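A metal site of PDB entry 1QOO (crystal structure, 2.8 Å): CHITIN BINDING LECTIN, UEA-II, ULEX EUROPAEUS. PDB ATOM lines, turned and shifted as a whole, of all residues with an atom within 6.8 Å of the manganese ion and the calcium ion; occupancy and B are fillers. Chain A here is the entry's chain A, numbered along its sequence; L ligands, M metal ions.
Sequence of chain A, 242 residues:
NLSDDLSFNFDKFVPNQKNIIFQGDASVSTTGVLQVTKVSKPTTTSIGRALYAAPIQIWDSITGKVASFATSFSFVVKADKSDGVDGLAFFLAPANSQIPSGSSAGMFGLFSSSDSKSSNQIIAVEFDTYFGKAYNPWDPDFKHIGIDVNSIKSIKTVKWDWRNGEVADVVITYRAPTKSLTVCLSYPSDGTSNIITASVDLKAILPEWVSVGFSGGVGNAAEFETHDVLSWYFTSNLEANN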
ATOM      1  N   ASP A  86      -7.736 -22.946  -6.928  1.00  0.00           N
ATOM      2  CA  ASP A  86      -7.169 -23.874  -7.894  1.00  0.00           C
ATOM      3  C   ASP A  86      -5.667 -24.059  -7.681  1.00  0.00           C
ATOM      4  O   ASP A  86      -5.102 -25.084  -8.072  1.00  0.00           O
ATOM      5  CB  ASP A  86      -7.362 -23.301  -9.298  1.00  0.00           C
ATOM      6  CG  ASP A  86      -8.475 -23.987 -10.038  1.00  0.00           C
ATOM      7  OD1 ASP A  86      -9.627 -23.556  -9.896  1.00  0.00           O
ATOM      8  OD2 ASP A  86      -8.171 -24.959 -10.758  1.00  0.00           O
ATOM      9  N   GLY A  87      -5.024 -23.052  -7.118  1.00  0.00           N
ATOM     10  CA  GLY A  87      -3.598 -23.138  -6.883  1.00  0.00           C
ATOM     11  C   GLY A  87      -2.906 -21.800  -7.025  1.00  0.00           C
ATOM     12  O   GLY A  87      -3.529 -20.775  -7.319  1.00  0.00           O
ATOM     13  N   ALA A 105      -8.869 -20.068 -14.237  1.00  0.00           N
ATOM     14  CA  ALA A 105      -8.226 -20.283 -12.948  1.00  0.00           C
ATOM     15  C   ALA A 105      -7.302 -21.499 -12.957  1.00  0.00           C
ATOM     16  O   ALA A 105      -6.210 -21.466 -12.376  1.00  0.00           O
ATOM     17  CB  ALA A 105      -9.277 -20.426 -11.872  1.00  0.00           C
ATOM     18  N   GLY A 106      -7.722 -22.548 -13.649  1.00  0.00           N
ATOM     19  CA  GLY A 106      -6.929 -23.763 -13.730  1.00  0.00           C
ATOM     20  C   GLY A 106      -5.631 -23.608 -14.475  1.00  0.00           C
ATOM     21  O   GLY A 106      -4.781 -24.516 -14.468  1.00  0.00           O
ATOM     22  N   MET A 107      -5.483 -22.482 -15.171  1.00  0.00           N
ATOM     23  CA  MET A 107      -4.270 -22.179 -15.910  1.00  0.00           C
ATOM     24  C   MET A 107      -3.512 -21.034 -15.242  1.00  0.00           C
ATOM     25  O   MET A 107      -2.535 -20.507 -15.777  1.00  0.00           O
ATOM     26  CB  MET A 107      -4.590 -21.897 -17.368  1.00  0.00           C
ATOM     27  CG  MET A 107      -5.189 -23.111 -18.030  1.00  0.00           C
ATOM     28  SD  MET A 107      -5.508 -22.949 -19.763  1.00  0.00           S
ATOM     29  CE  MET A 107      -6.982 -21.898 -19.768  1.00  0.00           C
ATOM     30  N   PHE A 108      -3.990 -20.665 -14.049  1.00  0.00           N
ATOM     31  CA  PHE A 108      -3.389 -19.621 -13.210  1.00  0.00           C
ATOM     32  C   PHE A 108      -3.154 -18.293 -13.912  1.00  0.00           C
ATOM     33  O   PHE A 108      -2.225 -17.564 -13.555  1.00  0.00           O
ATOM     34  CB  PHE A 108      -2.079 -20.147 -12.622  1.00  0.00           C
ATOM     35  CG  PHE A 108      -2.187 -21.523 -12.017  1.00  0.00           C
ATOM     36  CD1 PHE A 108      -3.015 -21.765 -10.920  1.00  0.00           C
ATOM     37  CD2 PHE A 108      -1.472 -22.594 -12.565  1.00  0.00           C
ATOM     38  CE1 PHE A 108      -3.131 -23.047 -10.380  1.00  0.00           C
ATOM     39  CE2 PHE A 108      -1.585 -23.885 -12.020  1.00  0.00           C
ATOM     40  CZ  PHE A 108      -2.409 -24.113 -10.924  1.00  0.00           C
ATOM     41  N   GLU A 126       4.217 -24.389 -10.229  1.00  0.00           N
ATOM     42  CA  GLU A 126       2.860 -24.390  -9.726  1.00  0.00           C
ATOM     43  C   GLU A 126       2.659 -25.207  -8.469  1.00  0.00           C
ATOM     44  O   GLU A 126       3.326 -26.215  -8.247  1.00  0.00           O
ATOM     45  CB  GLU A 126       1.898 -24.910 -10.809  1.00  0.00           C
ATOM     46  CG  GLU A 126       2.231 -26.293 -11.341  1.00  0.00           C
ATOM     47  CD  GLU A 126       1.082 -26.945 -12.079  1.00  0.00           C
ATOM     48  OE1 GLU A 126       0.645 -26.396 -13.114  1.00  0.00           O
ATOM     49  OE2 GLU A 126       0.600 -28.003 -11.630  1.00  0.00           O
ATOM     50  N   ASP A 128      -0.401 -26.664  -7.381  1.00  0.00           N
ATOM     51  CA  ASP A 128      -1.729 -27.076  -7.849  1.00  0.00           C
ATOM     52  C   ASP A 128      -2.575 -27.825  -6.829  1.00  0.00           C
ATOM     53  O   ASP A 128      -2.253 -28.952  -6.456  1.00  0.00           O
ATOM     54  CB  ASP A 128      -1.499 -27.965  -9.071  1.00  0.00           C
ATOM     55  CG  ASP A 128      -2.620 -27.918 -10.069  1.00  0.00           C
ATOM     56  OD1 ASP A 128      -3.772 -27.582  -9.692  1.00  0.00           O
ATOM     57  OD2 ASP A 128      -2.345 -28.256 -11.242  1.00  0.00           O
ATOM     58  N   THR A 129      -3.686 -27.220  -6.431  1.00  0.00           N
ATOM     59  CA  THR A 129      -4.574 -27.849  -5.444  1.00  0.00           C
ATOM     60  C   THR A 129      -5.732 -28.620  -6.060  1.00  0.00           C
ATOM     61  O   THR A 129      -6.335 -29.472  -5.406  1.00  0.00           O
ATOM     62  CB  THR A 129      -5.163 -26.809  -4.494  1.00  0.00           C
ATOM     63  OG1 THR A 129      -5.806 -25.794  -5.255  1.00  0.00           O
ATOM     64  CG2 THR A 129      -4.082 -26.197  -3.621  1.00  0.00           C
ATOM     65  N   TYR A 130      -6.091 -28.280  -7.294  1.00  0.00           N
ATOM     66  CA  TYR A 130      -7.178 -28.961  -7.992  1.00  0.00           C
ATOM     67  C   TYR A 130      -6.632 -29.825  -9.126  1.00  0.00           C
ATOM     68  O   TYR A 130      -5.897 -29.349 -10.003  1.00  0.00           O
ATOM     69  CB  TYR A 130      -8.186 -27.933  -8.533  1.00  0.00           C
ATOM     70  CG  TYR A 130      -9.316 -28.553  -9.338  1.00  0.00           C
ATOM     71  CD1 TYR A 130     -10.395 -29.175  -8.707  1.00  0.00           C
ATOM     72  CD2 TYR A 130      -9.290 -28.539 -10.735  1.00  0.00           C
ATOM     73  CE1 TYR A 130     -11.419 -29.764  -9.454  1.00  0.00           C
ATOM     74  CE2 TYR A 130     -10.308 -29.130 -11.490  1.00  0.00           C
ATOM     75  CZ  TYR A 130     -11.365 -29.738 -10.845  1.00  0.00           C
ATOM     76  OH  TYR A 130     -12.358 -30.345 -11.604  1.00  0.00           O
ATOM     77  N   PHE A 131      -7.025 -31.089  -9.121  1.00  0.00           N
ATOM     78  CA  PHE A 131      -6.574 -32.021 -10.133  1.00  0.00           C
ATOM     79  C   PHE A 131      -7.731 -32.808 -10.758  1.00  0.00           C
ATOM     80  O   PHE A 131      -7.521 -33.879 -11.349  1.00  0.00           O
ATOM     81  CB  PHE A 131      -5.542 -32.969  -9.517  1.00  0.00           C
ATOM     82  CG  PHE A 131      -6.043 -33.684  -8.289  1.00  0.00           C
ATOM     83  CD1 PHE A 131      -5.904 -33.122  -7.026  1.00  0.00           C
ATOM     84  CD2 PHE A 131      -6.665 -34.919  -8.396  1.00  0.00           C
ATOM     85  CE1 PHE A 131      -6.367 -33.772  -5.885  1.00  0.00           C
ATOM     86  CE2 PHE A 131      -7.140 -35.587  -7.261  1.00  0.00           C
ATOM     87  CZ  PHE A 131      -6.991 -35.014  -6.005  1.00  0.00           C
ATOM     88  N   GLY A 132      -8.945 -32.288 -10.631  1.00  0.00           N
ATOM     89  CA  GLY A 132     -10.115 -32.960 -11.177  1.00  0.00           C
ATOM     90  C   GLY A 132     -10.021 -33.222 -12.664  1.00  0.00           C
ATOM     91  O   GLY A 132      -9.866 -32.305 -13.459  1.00  0.00           O
ATOM     92  N   ASN A 136      -9.314 -30.378 -15.424  1.00  0.00           N
ATOM     93  CA  ASN A 136      -7.862 -30.387 -15.628  1.00  0.00           C
ATOM     94  C   ASN A 136      -7.380 -31.795 -15.982  1.00  0.00           C
ATOM     95  O   ASN A 136      -6.659 -32.433 -15.197  1.00  0.00           O
ATOM     96  CB  ASN A 136      -7.105 -29.945 -14.363  1.00  0.00           C
ATOM     97  CG  ASN A 136      -7.467 -28.549 -13.906  1.00  0.00           C
ATOM     98  OD1 ASN A 136      -7.179 -28.192 -12.765  1.00  0.00           O
ATOM     99  ND2 ASN A 136      -8.066 -27.756 -14.774  1.00  0.00           N
ATOM    100  N   TRP A 138      -5.053 -32.769 -17.700  1.00  0.00           N
ATOM    101  CA  TRP A 138      -3.591 -32.836 -17.770  1.00  0.00           C
ATOM    102  C   TRP A 138      -2.893 -33.101 -16.430  1.00  0.00           C
ATOM    103  O   TRP A 138      -1.711 -33.442 -16.405  1.00  0.00           O
ATOM    104  CB  TRP A 138      -3.071 -31.519 -18.336  1.00  0.00           C
ATOM    105  CG  TRP A 138      -3.572 -30.332 -17.557  1.00  0.00           C
ATOM    106  CD1 TRP A 138      -3.105 -29.872 -16.358  1.00  0.00           C
ATOM    107  CD2 TRP A 138      -4.666 -29.481 -17.919  1.00  0.00           C
ATOM    108  NE1 TRP A 138      -3.849 -28.795 -15.945  1.00  0.00           N
ATOM    109  CE2 TRP A 138      -4.814 -28.533 -16.877  1.00  0.00           C
ATOM    110  CE3 TRP A 138      -5.536 -29.427 -19.012  1.00  0.00           C
ATOM    111  CZ2 TRP A 138      -5.800 -27.541 -16.902  1.00  0.00           C
ATOM    112  CZ3 TRP A 138      -6.528 -28.433 -19.029  1.00  0.00           C
ATOM    113  CH2 TRP A 138      -6.640 -27.504 -17.981  1.00  0.00           C
ATOM    114  N   ASP A 139      -3.602 -32.898 -15.319  1.00  0.00           N
ATOM    115  CA  ASP A 139      -3.052 -33.074 -13.980  1.00  0.00           C
ATOM    116  C   ASP A 139      -2.998 -34.510 -13.495  1.00  0.00           C
ATOM    117  O   ASP A 139      -3.759 -35.352 -13.968  1.00  0.00           O
ATOM    118  CB  ASP A 139      -3.897 -32.278 -12.963  1.00  0.00           C
ATOM    119  CG  ASP A 139      -3.505 -30.807 -12.875  1.00  0.00           C
ATOM    120  OD1 ASP A 139      -2.316 -30.479 -13.109  1.00  0.00           O
ATOM    121  OD2 ASP A 139      -4.390 -29.979 -12.538  1.00  0.00           O
ATOM    122  N   PRO A 140      -2.044 -34.826 -12.598  1.00  0.00           N
ATOM    123  CA  PRO A 140      -1.890 -36.171 -12.022  1.00  0.00           C
ATOM    124  C   PRO A 140      -2.975 -36.325 -10.944  1.00  0.00           C
ATOM    125  O   PRO A 140      -3.660 -35.340 -10.620  1.00  0.00           O
ATOM    126  CB  PRO A 140      -0.481 -36.140 -11.435  1.00  0.00           C
ATOM    127  CG  PRO A 140      -0.297 -34.711 -11.088  1.00  0.00           C
ATOM    128  CD  PRO A 140      -0.856 -34.005 -12.286  1.00  0.00           C
ATOM    129  N   HIS A 144      -0.231 -31.283  -6.318  1.00  0.00           N
ATOM    130  CA  HIS A 144       1.167 -31.365  -6.710  1.00  0.00           C
ATOM    131  C   HIS A 144       1.940 -30.061  -6.885  1.00  0.00           C
ATOM    132  O   HIS A 144       1.358 -28.975  -6.911  1.00  0.00           O
ATOM    133  CB  HIS A 144       1.223 -32.133  -8.036  1.00  0.00           C
ATOM    134  CG  HIS A 144       0.300 -31.561  -9.080  1.00  0.00           C
ATOM    135  ND1 HIS A 144      -1.056 -31.760  -9.061  1.00  0.00           N
ATOM    136  CD2 HIS A 144       0.546 -30.750 -10.139  1.00  0.00           C
ATOM    137  CE1 HIS A 144      -1.619 -31.095 -10.052  1.00  0.00           C
ATOM    138  NE2 HIS A 144      -0.672 -30.471 -10.730  1.00  0.00           N
ATOM    139  N   ILE A 145       3.248 -30.210  -6.987  1.00  0.00           N
ATOM    140  CA  ILE A 145       4.149 -29.103  -7.278  1.00  0.00           C
ATOM    141  C   ILE A 145       4.594 -29.471  -8.684  1.00  0.00           C
ATOM    142  O   ILE A 145       4.970 -30.622  -8.934  1.00  0.00           O
ATOM    143  CB  ILE A 145       5.387 -29.084  -6.372  1.00  0.00           C
ATOM    144  CG1 ILE A 145       4.973 -28.923  -4.909  1.00  0.00           C
ATOM    145  CG2 ILE A 145       6.314 -27.952  -6.800  1.00  0.00           C
ATOM    146  CD1 ILE A 145       6.132 -28.989  -3.955  1.00  0.00           C
ATOM    147  N   GLY A 146       4.502 -28.541  -9.614  1.00  0.00           N
ATOM    148  CA  GLY A 146       4.902 -28.857 -10.977  1.00  0.00           C
ATOM    149  C   GLY A 146       5.760 -27.794 -11.617  1.00  0.00           C
ATOM    150  O   GLY A 146       5.660 -26.611 -11.285  1.00  0.00           O
ATOM    151  N   ASP A 148       6.377 -26.018 -14.937  1.00  0.00           N
ATOM    152  CA  ASP A 148       5.678 -25.785 -16.196  1.00  0.00           C
ATOM    153  C   ASP A 148       6.549 -25.046 -17.182  1.00  0.00           C
ATOM    154  O   ASP A 148       7.109 -23.989 -16.867  1.00  0.00           O
ATOM    155  CB  ASP A 148       4.397 -25.000 -15.950  1.00  0.00           C
ATOM    156  CG  ASP A 148       3.418 -25.723 -15.046  1.00  0.00           C
ATOM    157  OD1 ASP A 148       3.667 -26.885 -14.667  1.00  0.00           O
ATOM    158  OD2 ASP A 148       2.381 -25.127 -14.717  1.00  0.00           O
ATOM    159  N   ILE A 152       0.553 -25.773 -19.384  1.00  0.00           N
ATOM    160  CA  ILE A 152      -0.052 -26.050 -18.090  1.00  0.00           C
ATOM    161  C   ILE A 152       0.116 -27.521 -17.715  1.00  0.00           C
ATOM    162  O   ILE A 152      -0.173 -27.931 -16.588  1.00  0.00           O
ATOM    163  CB  ILE A 152      -1.549 -25.641 -18.083  1.00  0.00           C
ATOM    164  CG1 ILE A 152      -2.094 -25.599 -16.652  1.00  0.00           C
ATOM    165  CG2 ILE A 152      -2.351 -26.579 -18.943  1.00  0.00           C
ATOM    166  CD1 ILE A 152      -1.377 -24.634 -15.722  1.00  0.00           C
ATOM    167  N   LYS A 153       0.570 -28.314 -18.680  1.00  0.00           N
ATOM    168  CA  LYS A 153       0.831 -29.730 -18.476  1.00  0.00           C
ATOM    169  C   LYS A 153       2.313 -29.794 -18.092  1.00  0.00           C
ATOM    170  O   LYS A 153       3.191 -29.718 -18.938  1.00  0.00           O
ATOM    171  CB  LYS A 153       0.543 -30.517 -19.761  1.00  0.00           C
ATOM    172  CG  LYS A 153       0.843 -32.016 -19.687  1.00  0.00           C
ATOM    173  CD  LYS A 153       0.394 -32.719 -20.970  1.00  0.00           C
ATOM    174  CE  LYS A 153       1.022 -34.085 -21.124  1.00  0.00           C
ATOM    175  NZ  LYS A 153       0.806 -34.918 -19.913  1.00  0.00           N
ATOM    176  N   SER A 154       2.556 -29.873 -16.786  1.00  0.00           N
ATOM    177  CA  SER A 154       3.895 -29.901 -16.199  1.00  0.00           C
ATOM    178  C   SER A 154       4.800 -30.961 -16.812  1.00  0.00           C
ATOM    179  O   SER A 154       4.337 -32.042 -17.176  1.00  0.00           O
ATOM    180  CB  SER A 154       3.795 -30.161 -14.703  1.00  0.00           C
ATOM    181  OG  SER A 154       2.742 -29.417 -14.104  1.00  0.00           O
ATOM    182  N   THR A 157       6.300 -33.461 -12.065  1.00  0.00           N
ATOM    183  CA  THR A 157       5.506 -33.141 -10.892  1.00  0.00           C
ATOM    184  C   THR A 157       5.924 -34.016  -9.722  1.00  0.00           C
ATOM    185  O   THR A 157       6.660 -34.977  -9.888  1.00  0.00           O
ATOM    186  CB  THR A 157       3.981 -33.366 -11.118  1.00  0.00           C
ATOM    187  OG1 THR A 157       3.726 -34.753 -11.325  1.00  0.00           O
ATOM    188  CG2 THR A 157       3.495 -32.587 -12.316  1.00  0.00           C
HETATM  189  C1  LIG L   1     -13.715 -24.025 -13.514  1.00  0.00           C
HETATM  190  C2  LIG L   1     -12.611 -23.252 -14.236  1.00  0.00           C
HETATM  191  C3  LIG L   1     -11.337 -24.092 -14.323  1.00  0.00           C
HETATM  192  C4  LIG L   1     -10.959 -24.608 -12.935  1.00  0.00           C
HETATM  193  C5  LIG L   1     -12.145 -25.350 -12.330  1.00  0.00           C
HETATM  194  C6  LIG L   1     -11.873 -25.911 -10.960  1.00  0.00           C
HETATM  195  C7  LIG L   1     -13.630 -21.694 -15.772  1.00  0.00           C
HETATM  196  C8  LIG L   1     -14.093 -21.395 -17.187  1.00  0.00           C
HETATM  197  N1  LIG L   1     -13.087 -22.892 -15.561  1.00  0.00           N
HETATM  198  O1  LIG L   1     -14.808 -23.197 -13.316  1.00  0.00           O
HETATM  199  O2  LIG L   1     -10.261 -23.307 -14.855  1.00  0.00           O
HETATM  200  O3  LIG L   1      -9.850 -25.525 -13.039  1.00  0.00           O
HETATM  201  O4  LIG L   1     -13.262 -24.459 -12.227  1.00  0.00           O
HETATM  202  O5  LIG L   1     -11.956 -24.886  -9.975  1.00  0.00           O
HETATM  203  O6  LIG L   1     -13.757 -20.846 -14.882  1.00  0.00           O
HETATM  204 MN    MN M   1      -0.839 -29.234 -12.464  1.00  0.00          MN
HETATM  205 CA    CA M   2      -5.054 -27.657 -11.650  1.00  0.00          CA
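The manganese ion is bound by OD1 of Asp 139, OE2 of Glu 126, NE2 of His 144 and OD2 of Asp 128.
The manganese ion has four donor atoms within binding distance.
Along chain A the residues within 4 Å of the calcium ion span positions 128 to 139.
The nearest printed residue that does not touch the calcium ion is Asp 86 (4.2 Å).
O3 of the ligand sits at hydrogen-bond distance from ND2 of Asn 136, 3.3 Å away.
N of Gly 106 lies within hydrogen-bond range of O2 of the ligand, 2.9 Å away.
OD1 of Asp 86 sits at hydrogen-bond distance from O5 of the ligand (2.7 Å).
Ser 154 touches the manganese ion.
The nearest printed residue that does not touch the manganese ion is Ile 152 (4.4 Å).
The calcium ion is bound by OD1 of Asp 128 (2.3 Å), OD1 of Asn 136 (2.5 Å), O of Tyr 130 (2.5 Å), OD2 of Asp 139 (2.6 Å) and OD2 of Asp 128 (2.8 Å).
The calcium ion has five donor atoms within binding distance.
The side-chain hydroxyl (OG) of Ser 154 is in hydrogen-bond range of the side-chain carboxylate (OD1) of Asp 148, at 2.8 Å.
The side-chain carboxylate (OE1) of Glu 126 sits close to the side-chain carboxylate (OD2) of Asp 148 (2.7 Å).
The backbone NH of Glu 126 lies within hydrogen-bond range of the backbone carbonyl oxygen of Gly 146, 2.9 Å away.
N of Tyr 130 lies within hydrogen-bond range of O of Asp 86 (3.4 Å).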
